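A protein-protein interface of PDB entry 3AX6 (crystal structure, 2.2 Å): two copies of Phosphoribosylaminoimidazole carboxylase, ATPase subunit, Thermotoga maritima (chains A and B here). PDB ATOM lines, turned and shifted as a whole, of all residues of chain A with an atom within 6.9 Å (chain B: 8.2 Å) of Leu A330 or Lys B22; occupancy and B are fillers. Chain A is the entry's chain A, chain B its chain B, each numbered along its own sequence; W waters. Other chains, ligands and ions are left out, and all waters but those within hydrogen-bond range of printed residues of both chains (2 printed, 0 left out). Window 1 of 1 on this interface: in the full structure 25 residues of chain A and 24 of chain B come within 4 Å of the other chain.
The backbone carbonyl oxygen of Leu A328 sits at hydrogen-bond distance from the guanidinium group of Arg B283, 3.0 Å away.
The backbone carbonyl oxygen (O) of Leu A330 is in hydrogen-bond range of the side-chain amino group (NZ) of Lys B22 (3.1 Å).
N of Phe A332 lies within hydrogen-bond range of O of Lys B22 (2.8 Å).
The side-chain carboxylate (OE2) of Glu B279 lies within salt-bridge range of the guanidinium group (NH2) of Arg B283, 2.8 Å away.
N of His A331 sits at hydrogen-bond distance from O of His A346 (2.8 Å).
Among the printed residues, pairs that only touch across the chains: Leu A316 with Met B23 (3.96 Å), Leu A323 with Arg B283 (3.6 Å), His A331 with Lys B22 (3.7 Å), Phe A332 with Lys B21 (3.7 Å) and Phe A332 with Gly B24 (3.6 Å).
Leu A330 touches just one residue of chain B: Lys B22.
Lys B22 touches just these residues of chain A: Leu A330 (3.1 Å), His A331 (3.7 Å) and Phe A332 (2.8 Å).
Ser A329 touches none of the printed residues of chain B.
Of the printed residues of chain B, Phe A332 touches Lys B21, Lys B22 and Gly B24.
Printed residues of chain A within 4 Å of Arg B283: Leu A323 and Leu A328.
Of the printed residues of chain A, Lys B21 touches Phe A332 (3.7 Å).
Of the printed residues of chain B, His A331 touches Lys B22 (3.7 Å).
Leu B18 touches none of the printed residues of chain A.
Gly A345 touches none of the printed residues of chain B.
The nearest residue of chain A that does not touch Lys B22 is Glu A271 (4.5 Å).
The nearest printed residue of chain B that does not touch Leu A328 is Glu B279 (4.8 Å).
Printed residues of chain A that touch a printed residue of chain B: Leu A316, Leu A323, Leu A328, Leu A330, His A331 and Phe A332.
Among the printed residues, 8 pairs touch across the chains.
Among the printed residues, no Asp or Glu carboxylate lies within 4 Å of a Lys or Arg side-chain nitrogen of the other chain.
No position is printed for both chains.
Water W1 lies within hydrogen-bond range of O of Leu A328 (2.6 Å), NH1 of Arg B283 (2.9 Å) and O of Leu A323 (3.1 Å).
Water W2 lies within hydrogen-bond range of N of Leu A330 (3.2 Å) and OE2 of Glu B279 (3.3 Å).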
ATOM      1  N   ILE A 270     -32.587  -8.243  35.902  1.00  0.00           N
ATOM      2  CA  ILE A 270     -32.251  -8.098  34.484  1.00  0.00           C
ATOM      3  C   ILE A 270     -31.129  -9.037  34.074  1.00  0.00           C
ATOM      4  O   ILE A 270     -31.132  -9.576  32.965  1.00  0.00           O
ATOM      5  CB  ILE A 270     -31.810  -6.652  34.158  1.00  0.00           C
ATOM      6  CG1 ILE A 270     -32.968  -5.687  34.410  1.00  0.00           C
ATOM      7  CG2 ILE A 270     -31.345  -6.552  32.709  1.00  0.00           C
ATOM      8  CD1 ILE A 270     -32.565  -4.225  34.379  1.00  0.00           C
ATOM      9  N   GLU A 271     -30.185  -9.245  34.988  1.00  0.00           N
ATOM     10  CA  GLU A 271     -29.031 -10.093  34.724  1.00  0.00           C
ATOM     11  C   GLU A 271     -29.103 -11.504  35.296  1.00  0.00           C
ATOM     12  O   GLU A 271     -28.466 -12.404  34.763  1.00  0.00           O
ATOM     13  CB  GLU A 271     -27.758  -9.453  35.290  1.00  0.00           C
ATOM     14  CG  GLU A 271     -27.612  -7.945  35.123  1.00  0.00           C
ATOM     15  CD  GLU A 271     -27.441  -7.512  33.680  1.00  0.00           C
ATOM     16  OE1 GLU A 271     -26.912  -8.307  32.867  1.00  0.00           O
ATOM     17  OE2 GLU A 271     -27.825  -6.363  33.365  1.00  0.00           O
ATOM     18  N   LEU A 304     -23.815   3.283  40.273  1.00  0.00           N
ATOM     19  CA  LEU A 304     -22.730   4.146  39.849  1.00  0.00           C
ATOM     20  C   LEU A 304     -23.269   5.556  40.002  1.00  0.00           C
ATOM     21  O   LEU A 304     -24.260   5.912  39.366  1.00  0.00           O
ATOM     22  CB  LEU A 304     -22.364   3.895  38.389  1.00  0.00           C
ATOM     23  CG  LEU A 304     -21.470   2.702  38.071  1.00  0.00           C
ATOM     24  CD1 LEU A 304     -21.179   2.689  36.586  1.00  0.00           C
ATOM     25  CD2 LEU A 304     -20.173   2.804  38.850  1.00  0.00           C
ATOM     26  N   LEU A 316     -16.275   7.898  31.880  1.00  0.00           N
ATOM     27  CA  LEU A 316     -15.989   6.736  32.705  1.00  0.00           C
ATOM     28  C   LEU A 316     -14.509   6.430  32.892  1.00  0.00           C
ATOM     29  O   LEU A 316     -13.696   6.654  31.997  1.00  0.00           O
ATOM     30  CB  LEU A 316     -16.664   5.508  32.105  1.00  0.00           C
ATOM     31  CG  LEU A 316     -18.185   5.461  32.137  1.00  0.00           C
ATOM     32  CD1 LEU A 316     -18.675   4.395  31.168  1.00  0.00           C
ATOM     33  CD2 LEU A 316     -18.654   5.168  33.554  1.00  0.00           C
ATOM     34  N   LEU A 319     -13.080   1.290  33.159  1.00  0.00           N
ATOM     35  CA  LEU A 319     -13.830   0.342  32.349  1.00  0.00           C
ATOM     36  C   LEU A 319     -13.054  -0.922  32.011  1.00  0.00           C
ATOM     37  O   LEU A 319     -13.536  -2.019  32.273  1.00  0.00           O
ATOM     38  CB  LEU A 319     -14.331   0.996  31.055  1.00  0.00           C
ATOM     39  CG  LEU A 319     -15.305   0.113  30.257  1.00  0.00           C
ATOM     40  CD1 LEU A 319     -16.485  -0.254  31.135  1.00  0.00           C
ATOM     41  CD2 LEU A 319     -15.782   0.830  29.004  1.00  0.00           C
ATOM     42  N   LEU A 323     -14.041  -4.437  33.375  1.00  0.00           N
ATOM     43  CA  LEU A 323     -14.539  -5.480  32.488  1.00  0.00           C
ATOM     44  C   LEU A 323     -13.634  -6.704  32.477  1.00  0.00           C
ATOM     45  O   LEU A 323     -14.004  -7.749  31.946  1.00  0.00           O
ATOM     46  CB  LEU A 323     -14.710  -4.948  31.067  1.00  0.00           C
ATOM     47  CG  LEU A 323     -15.881  -4.000  30.788  1.00  0.00           C
ATOM     48  CD1 LEU A 323     -15.880  -3.651  29.300  1.00  0.00           C
ATOM     49  CD2 LEU A 323     -17.215  -4.664  31.179  1.00  0.00           C
ATOM     50  N   LEU A 328     -18.751  -9.379  35.414  1.00  0.00           N
ATOM     51  CA  LEU A 328     -19.055  -7.955  35.565  1.00  0.00           C
ATOM     52  C   LEU A 328     -19.633  -7.404  34.261  1.00  0.00           C
ATOM     53  O   LEU A 328     -19.055  -7.588  33.194  1.00  0.00           O
ATOM     54  CB  LEU A 328     -17.768  -7.186  35.919  1.00  0.00           C
ATOM     55  CG  LEU A 328     -17.612  -5.668  36.186  1.00  0.00           C
ATOM     56  CD1 LEU A 328     -18.510  -4.834  35.285  1.00  0.00           C
ATOM     57  CD2 LEU A 328     -17.882  -5.356  37.640  1.00  0.00           C
ATOM     58  N   SER A 329     -20.785  -6.748  34.344  1.00  0.00           N
ATOM     59  CA  SER A 329     -21.386  -6.132  33.170  1.00  0.00           C
ATOM     60  C   SER A 329     -21.784  -4.716  33.585  1.00  0.00           C
ATOM     61  O   SER A 329     -22.092  -4.466  34.752  1.00  0.00           O
ATOM     62  CB  SER A 329     -22.608  -6.920  32.686  1.00  0.00           C
ATOM     63  OG  SER A 329     -23.667  -6.858  33.619  1.00  0.00           O
ATOM     64  N   LEU A 330     -21.773  -3.790  32.635  1.00  0.00           N
ATOM     65  CA  LEU A 330     -22.098  -2.408  32.934  1.00  0.00           C
ATOM     66  C   LEU A 330     -23.393  -1.895  32.319  1.00  0.00           C
ATOM     67  O   LEU A 330     -23.714  -2.193  31.172  1.00  0.00           O
ATOM     68  CB  LEU A 330     -20.944  -1.515  32.493  1.00  0.00           C
ATOM     69  CG  LEU A 330     -21.251  -0.022  32.442  1.00  0.00           C
ATOM     70  CD1 LEU A 330     -21.602   0.484  33.837  1.00  0.00           C
ATOM     71  CD2 LEU A 330     -20.047   0.717  31.882  1.00  0.00           C
ATOM     72  N   HIS A 331     -24.128  -1.108  33.096  1.00  0.00           N
ATOM     73  CA  HIS A 331     -25.379  -0.523  32.639  1.00  0.00           C
ATOM     74  C   HIS A 331     -25.345   0.983  32.912  1.00  0.00           C
ATOM     75  O   HIS A 331     -25.857   1.457  33.916  1.00  0.00           O
ATOM     76  CB  HIS A 331     -26.561  -1.153  33.371  1.00  0.00           C
ATOM     77  CG  HIS A 331     -27.874  -0.924  32.696  1.00  0.00           C
ATOM     78  ND1 HIS A 331     -28.177   0.252  32.040  1.00  0.00           N
ATOM     79  CD2 HIS A 331     -28.977  -1.705  32.599  1.00  0.00           C
ATOM     80  CE1 HIS A 331     -29.409   0.186  31.571  1.00  0.00           C
ATOM     81  NE2 HIS A 331     -29.917  -0.990  31.896  1.00  0.00           N
ATOM     82  N   PHE A 332     -24.731   1.725  32.002  1.00  0.00           N
ATOM     83  CA  PHE A 332     -24.602   3.173  32.116  1.00  0.00           C
ATOM     84  C   PHE A 332     -25.829   3.837  31.489  1.00  0.00           C
ATOM     85  O   PHE A 332     -26.116   3.619  30.313  1.00  0.00           O
ATOM     86  CB  PHE A 332     -23.331   3.605  31.382  1.00  0.00           C
ATOM     87  CG  PHE A 332     -23.035   5.069  31.465  1.00  0.00           C
ATOM     88  CD1 PHE A 332     -22.476   5.614  32.608  1.00  0.00           C
ATOM     89  CD2 PHE A 332     -23.278   5.898  30.375  1.00  0.00           C
ATOM     90  CE1 PHE A 332     -22.151   6.965  32.669  1.00  0.00           C
ATOM     91  CE2 PHE A 332     -22.960   7.250  30.421  1.00  0.00           C
ATOM     92  CZ  PHE A 332     -22.392   7.787  31.571  1.00  0.00           C
ATOM     93  N   TYR A 333     -26.565   4.625  32.271  1.00  0.00           N
ATOM     94  CA  TYR A 333     -27.743   5.303  31.740  1.00  0.00           C
ATOM     95  C   TYR A 333     -27.216   6.516  30.973  1.00  0.00           C
ATOM     96  O   TYR A 333     -26.263   7.164  31.409  1.00  0.00           O
ATOM     97  CB  TYR A 333     -28.678   5.774  32.861  1.00  0.00           C
ATOM     98  CG  TYR A 333     -28.888   4.799  34.004  1.00  0.00           C
ATOM     99  CD1 TYR A 333     -29.026   3.428  33.774  1.00  0.00           C
ATOM    100  CD2 TYR A 333     -28.978   5.256  35.320  1.00  0.00           C
ATOM    101  CE1 TYR A 333     -29.244   2.532  34.831  1.00  0.00           C
ATOM    102  CE2 TYR A 333     -29.202   4.369  36.388  1.00  0.00           C
ATOM    103  CZ  TYR A 333     -29.330   3.010  36.135  1.00  0.00           C
ATOM    104  OH  TYR A 333     -29.523   2.135  37.183  1.00  0.00           O
ATOM    105  N   GLY A 334     -27.830   6.829  29.840  1.00  0.00           N
ATOM    106  CA  GLY A 334     -27.362   7.955  29.056  1.00  0.00           C
ATOM    107  C   GLY A 334     -27.806   9.325  29.537  1.00  0.00           C
ATOM    108  O   GLY A 334     -28.554  10.013  28.844  1.00  0.00           O
ATOM    109  N   GLY A 345     -25.926   5.225  36.720  1.00  0.00           N
ATOM    110  CA  GLY A 345     -26.063   3.869  36.224  1.00  0.00           C
ATOM    111  C   GLY A 345     -25.752   2.854  37.300  1.00  0.00           C
ATOM    112  O   GLY A 345     -25.720   3.183  38.490  1.00  0.00           O
ATOM    113  N   HIS A 346     -25.549   1.612  36.885  1.00  0.00           N
ATOM    114  CA  HIS A 346     -25.203   0.554  37.814  1.00  0.00           C
ATOM    115  C   HIS A 346     -24.411  -0.505  37.066  1.00  0.00           C
ATOM    116  O   HIS A 346     -24.376  -0.510  35.833  1.00  0.00           O
ATOM    117  CB  HIS A 346     -26.465  -0.074  38.455  1.00  0.00           C
ATOM    118  CG  HIS A 346     -27.301  -0.898  37.516  1.00  0.00           C
ATOM    119  ND1 HIS A 346     -28.320  -0.363  36.757  1.00  0.00           N
ATOM    120  CD2 HIS A 346     -27.272  -2.221  37.223  1.00  0.00           C
ATOM    121  CE1 HIS A 346     -28.883  -1.320  36.038  1.00  0.00           C
ATOM    122  NE2 HIS A 346     -28.266  -2.457  36.301  1.00  0.00           N
ATOM    123  N   PHE A 347     -23.735  -1.370  37.813  1.00  0.00           N
ATOM    124  CA  PHE A 347     -23.001  -2.461  37.215  1.00  0.00           C
ATOM    125  C   PHE A 347     -23.356  -3.673  38.051  1.00  0.00           C
ATOM    126  O   PHE A 347     -23.732  -3.539  39.218  1.00  0.00           O
ATOM    127  CB  PHE A 347     -21.483  -2.179  37.158  1.00  0.00           C
ATOM    128  CG  PHE A 347     -20.781  -2.196  38.489  1.00  0.00           C
ATOM    129  CD1 PHE A 347     -20.400  -3.397  39.078  1.00  0.00           C
ATOM    130  CD2 PHE A 347     -20.439  -1.001  39.120  1.00  0.00           C
ATOM    131  CE1 PHE A 347     -19.684  -3.409  40.272  1.00  0.00           C
ATOM    132  CE2 PHE A 347     -19.725  -0.997  40.313  1.00  0.00           C
ATOM    133  CZ  PHE A 347     -19.342  -2.198  40.893  1.00  0.00           C
ATOM    134  N   THR A 348     -23.286  -4.851  37.445  1.00  0.00           N
ATOM    135  CA  THR A 348     -23.643  -6.084  38.129  1.00  0.00           C
ATOM    136  C   THR A 348     -22.554  -7.128  37.972  1.00  0.00           C
ATOM    137  O   THR A 348     -21.864  -7.183  36.957  1.00  0.00           O
ATOM    138  CB  THR A 348     -24.948  -6.662  37.561  1.00  0.00           C
ATOM    139  OG1 THR A 348     -26.002  -5.701  37.704  1.00  0.00           O
ATOM    140  CG2 THR A 348     -25.332  -7.920  38.301  1.00  0.00           C
ATOM    141  N   LEU A 368     -14.518   1.450  38.871  1.00  0.00           N
ATOM    142  CA  LEU A 368     -15.460   2.115  37.981  1.00  0.00           C
ATOM    143  C   LEU A 368     -15.898   3.433  38.581  1.00  0.00           C
ATOM    144  O   LEU A 368     -16.356   3.472  39.720  1.00  0.00           O
ATOM    145  CB  LEU A 368     -16.693   1.240  37.756  1.00  0.00           C
ATOM    146  CG  LEU A 368     -16.729   0.435  36.461  1.00  0.00           C
ATOM    147  CD1 LEU A 368     -18.038  -0.339  36.367  1.00  0.00           C
ATOM    148  CD2 LEU A 368     -16.576   1.383  35.280  1.00  0.00           C
ATOM    149  N   MET B  15     -30.103  -3.278  18.013  1.00  0.00           N
ATOM    150  CA  MET B  15     -29.705  -4.059  19.174  1.00  0.00           C
ATOM    151  C   MET B  15     -28.261  -3.710  19.526  1.00  0.00           C
ATOM    152  O   MET B  15     -27.892  -3.652  20.700  1.00  0.00           O
ATOM    153  CB  MET B  15     -29.858  -5.554  18.869  1.00  0.00           C
ATOM    154  CG  MET B  15     -31.308  -5.956  18.554  1.00  0.00           C
ATOM    155  SD  MET B  15     -31.645  -7.802  17.963  1.00  0.00           S
ATOM    156  CE  MET B  15     -31.893  -8.609  19.710  1.00  0.00           C
ATOM    157  N   MET B  16     -27.455  -3.458  18.501  1.00  0.00           N
ATOM    158  CA  MET B  16     -26.051  -3.098  18.678  1.00  0.00           C
ATOM    159  C   MET B  16     -25.866  -1.740  19.362  1.00  0.00           C
ATOM    160  O   MET B  16     -25.111  -1.618  20.332  1.00  0.00           O
ATOM    161  CB  MET B  16     -25.335  -3.046  17.322  1.00  0.00           C
ATOM    162  CG  MET B  16     -24.985  -4.391  16.710  1.00  0.00           C
ATOM    163  SD  MET B  16     -24.040  -4.172  15.021  1.00  0.00           S
ATOM    164  CE  MET B  16     -22.614  -3.069  15.652  1.00  0.00           C
ATOM    165  N   THR B  17     -26.534  -0.718  18.838  1.00  0.00           N
ATOM    166  CA  THR B  17     -26.414   0.623  19.394  1.00  0.00           C
ATOM    167  C   THR B  17     -26.938   0.653  20.830  1.00  0.00           C
ATOM    168  O   THR B  17     -26.410   1.360  21.678  1.00  0.00           O
ATOM    169  CB  THR B  17     -27.165   1.664  18.518  1.00  0.00           C
ATOM    170  OG1 THR B  17     -28.554   1.686  18.860  1.00  0.00           O
ATOM    171  CG2 THR B  17     -27.033   1.302  17.046  1.00  0.00           C
ATOM    172  N   LEU B  18     -27.966  -0.144  21.099  1.00  0.00           N
ATOM    173  CA  LEU B  18     -28.550  -0.229  22.431  1.00  0.00           C
ATOM    174  C   LEU B  18     -27.532  -0.738  23.451  1.00  0.00           C
ATOM    175  O   LEU B  18     -27.425  -0.194  24.551  1.00  0.00           O
ATOM    176  CB  LEU B  18     -29.763  -1.159  22.395  1.00  0.00           C
ATOM    177  CG  LEU B  18     -31.136  -0.570  22.725  1.00  0.00           C
ATOM    178  CD1 LEU B  18     -31.245   0.866  22.244  1.00  0.00           C
ATOM    179  CD2 LEU B  18     -32.205  -1.439  22.082  1.00  0.00           C
ATOM    180  N   GLU B  19     -26.781  -1.779  23.092  1.00  0.00           N
ATOM    181  CA  GLU B  19     -25.772  -2.331  23.996  1.00  0.00           C
ATOM    182  C   GLU B  19     -24.582  -1.387  24.087  1.00  0.00           C
ATOM    183  O   GLU B  19     -23.988  -1.229  25.148  1.00  0.00           O
ATOM    184  CB  GLU B  19     -25.297  -3.712  23.527  1.00  0.00           C
ATOM    185  CG  GLU B  19     -26.251  -4.862  23.856  1.00  0.00           C
ATOM    186  CD  GLU B  19     -26.450  -5.065  25.356  1.00  0.00           C
ATOM    187  OE1 GLU B  19     -25.442  -5.129  26.093  1.00  0.00           O
ATOM    188  OE2 GLU B  19     -27.618  -5.164  25.796  1.00  0.00           O
ATOM    189  N   ALA B  20     -24.245  -0.758  22.970  1.00  0.00           N
ATOM    190  CA  ALA B  20     -23.134   0.182  22.927  1.00  0.00           C
ATOM    191  C   ALA B  20     -23.368   1.390  23.851  1.00  0.00           C
ATOM    192  O   ALA B  20     -22.477   1.796  24.606  1.00  0.00           O
ATOM    193  CB  ALA B  20     -22.926   0.657  21.500  1.00  0.00           C
ATOM    194  N   LYS B  21     -24.561   1.971  23.784  1.00  0.00           N
ATOM    195  CA  LYS B  21     -24.856   3.130  24.613  1.00  0.00           C
ATOM    196  C   LYS B  21     -24.933   2.692  26.064  1.00  0.00           C
ATOM    197  O   LYS B  21     -24.587   3.448  26.965  1.00  0.00           O
ATOM    198  CB  LYS B  21     -26.172   3.785  24.185  1.00  0.00           C
ATOM    199  CG  LYS B  21     -26.176   4.285  22.747  1.00  0.00           C
ATOM    200  CD  LYS B  21     -27.270   5.316  22.517  1.00  0.00           C
ATOM    201  CE  LYS B  21     -27.011   6.574  23.338  1.00  0.00           C
ATOM    202  NZ  LYS B  21     -27.973   7.678  23.049  1.00  0.00           N
ATOM    203  N   LYS B  22     -25.371   1.457  26.273  1.00  0.00           N
ATOM    204  CA  LYS B  22     -25.492   0.893  27.610  1.00  0.00           C
ATOM    205  C   LYS B  22     -24.099   0.804  28.235  1.00  0.00           C
ATOM    206  O   LYS B  22     -23.946   0.817  29.457  1.00  0.00           O
ATOM    207  CB  LYS B  22     -26.128  -0.502  27.520  1.00  0.00           C
ATOM    208  CG  LYS B  22     -26.897  -0.926  28.750  1.00  0.00           C
ATOM    209  CD  LYS B  22     -27.643  -2.234  28.523  1.00  0.00           C
ATOM    210  CE  LYS B  22     -26.740  -3.448  28.716  1.00  0.00           C
ATOM    211  NZ  LYS B  22     -26.286  -3.622  30.131  1.00  0.00           N
ATOM    212  N   MET B  23     -23.079   0.727  27.387  1.00  0.00           N
ATOM    213  CA  MET B  23     -21.708   0.627  27.866  1.00  0.00           C
ATOM    214  C   MET B  23     -21.069   2.009  27.888  1.00  0.00           C
ATOM    215  O   MET B  23     -19.869   2.151  28.129  1.00  0.00           O
ATOM    216  CB  MET B  23     -20.910  -0.320  26.971  1.00  0.00           C
ATOM    217  CG  MET B  23     -19.731  -0.995  27.662  1.00  0.00           C
ATOM    218  SD  MET B  23     -18.941  -2.393  26.566  1.00  0.00           S
ATOM    219  CE  MET B  23     -20.517  -3.483  26.385  1.00  0.00           C
ATOM    220  N   GLY B  24     -21.892   3.022  27.625  1.00  0.00           N
ATOM    221  CA  GLY B  24     -21.424   4.396  27.634  1.00  0.00           C
ATOM    222  C   GLY B  24     -20.805   4.944  26.358  1.00  0.00           C
ATOM    223  O   GLY B  24     -20.021   5.889  26.419  1.00  0.00           O
ATOM    224  N   PHE B  25     -21.139   4.379  25.204  1.00  0.00           N
ATOM    225  CA  PHE B  25     -20.575   4.876  23.954  1.00  0.00           C
ATOM    226  C   PHE B  25     -21.574   5.715  23.168  1.00  0.00           C
ATOM    227  O   PHE B  25     -22.783   5.564  23.331  1.00  0.00           O
ATOM    228  CB  PHE B  25     -20.108   3.708  23.071  1.00  0.00           C
ATOM    229  CG  PHE B  25     -18.923   2.964  23.618  1.00  0.00           C
ATOM    230  CD1 PHE B  25     -17.695   3.600  23.767  1.00  0.00           C
ATOM    231  CD2 PHE B  25     -19.045   1.629  24.012  1.00  0.00           C
ATOM    232  CE1 PHE B  25     -16.608   2.921  24.306  1.00  0.00           C
ATOM    233  CE2 PHE B  25     -17.971   0.941  24.550  1.00  0.00           C
ATOM    234  CZ  PHE B  25     -16.748   1.584  24.701  1.00  0.00           C
ATOM    235  N   TYR B  26     -21.051   6.597  22.315  1.00  0.00           N
ATOM    236  CA  TYR B  26     -21.862   7.460  21.446  1.00  0.00           C
ATOM    237  C   TYR B  26     -21.996   6.691  20.127  1.00  0.00           C
ATOM    238  O   TYR B  26     -21.010   6.143  19.636  1.00  0.00           O
ATOM    239  CB  TYR B  26     -21.118   8.778  21.207  1.00  0.00           C
ATOM    240  CG  TYR B  26     -21.882   9.834  20.441  1.00  0.00           C
ATOM    241  CD1 TYR B  26     -22.585  10.836  21.107  1.00  0.00           C
ATOM    242  CD2 TYR B  26     -21.869   9.855  19.049  1.00  0.00           C
ATOM    243  CE1 TYR B  26     -23.250  11.837  20.404  1.00  0.00           C
ATOM    244  CE2 TYR B  26     -22.529  10.846  18.337  1.00  0.00           C
ATOM    245  CZ  TYR B  26     -23.216  11.837  19.017  1.00  0.00           C
ATOM    246  OH  TYR B  26     -23.848  12.838  18.307  1.00  0.00           O
ATOM    247  N   VAL B  27     -23.190   6.643  19.545  1.00  0.00           N
ATOM    248  CA  VAL B  27     -23.369   5.892  18.302  1.00  0.00           C
ATOM    249  C   VAL B  27     -23.984   6.655  17.122  1.00  0.00           C
ATOM    250  O   VAL B  27     -25.008   7.321  17.263  1.00  0.00           O
ATOM    251  CB  VAL B  27     -24.232   4.631  18.546  1.00  0.00           C
ATOM    252  CG1 VAL B  27     -23.738   3.890  19.772  1.00  0.00           C
ATOM    253  CG2 VAL B  27     -25.679   5.018  18.718  1.00  0.00           C
ATOM    254  N   SER B 276     -24.568 -11.327  26.141  1.00  0.00           N
ATOM    255  CA  SER B 276     -25.206 -11.467  24.849  1.00  0.00           C
ATOM    256  C   SER B 276     -24.179 -11.315  23.735  1.00  0.00           C
ATOM    257  O   SER B 276     -23.078 -10.796  23.951  1.00  0.00           O
ATOM    258  CB  SER B 276     -26.282 -10.398  24.684  1.00  0.00           C
ATOM    259  OG  SER B 276     -25.698  -9.129  24.451  1.00  0.00           O
ATOM    260  N   GLU B 279     -23.344  -7.694  23.333  1.00  0.00           N
ATOM    261  CA  GLU B 279     -22.428  -7.044  24.247  1.00  0.00           C
ATOM    262  C   GLU B 279     -21.008  -7.443  23.877  1.00  0.00           C
ATOM    263  O   GLU B 279     -20.091  -6.638  24.007  1.00  0.00           O
ATOM    264  CB  GLU B 279     -22.699  -7.429  25.702  1.00  0.00           C
ATOM    265  CG  GLU B 279     -21.974  -6.519  26.688  1.00  0.00           C
ATOM    266  CD  GLU B 279     -21.995  -7.039  28.121  1.00  0.00           C
ATOM    267  OE1 GLU B 279     -23.071  -7.468  28.591  1.00  0.00           O
ATOM    268  OE2 GLU B 279     -20.931  -7.009  28.781  1.00  0.00           O
ATOM    269  N   ILE B 282     -19.534  -5.422  20.909  1.00  0.00           N
ATOM    270  CA  ILE B 282     -19.081  -4.089  21.298  1.00  0.00           C
ATOM    271  C   ILE B 282     -17.761  -4.222  22.039  1.00  0.00           C
ATOM    272  O   ILE B 282     -16.804  -3.499  21.748  1.00  0.00           O
ATOM    273  CB  ILE B 282     -20.103  -3.358  22.207  1.00  0.00           C
ATOM    274  CG1 ILE B 282     -21.453  -3.227  21.489  1.00  0.00           C
ATOM    275  CG2 ILE B 282     -19.591  -1.970  22.553  1.00  0.00           C
ATOM    276  CD1 ILE B 282     -21.369  -2.577  20.108  1.00  0.00           C
ATOM    277  N   ARG B 283     -17.708  -5.150  22.991  1.00  0.00           N
ATOM    278  CA  ARG B 283     -16.477  -5.370  23.729  1.00  0.00           C
ATOM    279  C   ARG B 283     -15.368  -5.689  22.734  1.00  0.00           C
ATOM    280  O   ARG B 283     -14.288  -5.106  22.787  1.00  0.00           O
ATOM    281  CB  ARG B 283     -16.612  -6.546  24.688  1.00  0.00           C
ATOM    282  CG  ARG B 283     -17.526  -6.322  25.887  1.00  0.00           C
ATOM    283  CD  ARG B 283     -17.194  -7.360  26.946  1.00  0.00           C
ATOM    284  NE  ARG B 283     -18.129  -7.374  28.061  1.00  0.00           N
ATOM    285  CZ  ARG B 283     -17.809  -7.788  29.280  1.00  0.00           C
ATOM    286  NH1 ARG B 283     -16.577  -8.213  29.535  1.00  0.00           N
ATOM    287  NH2 ARG B 283     -18.721  -7.784  30.241  1.00  0.00           N
HETATM  288  O   HOH W   1     -16.904  -8.834  32.314  1.00  0.00           O
HETATM  289  O   HOH W   2     -21.237  -3.783  29.455  1.00  0.00           O
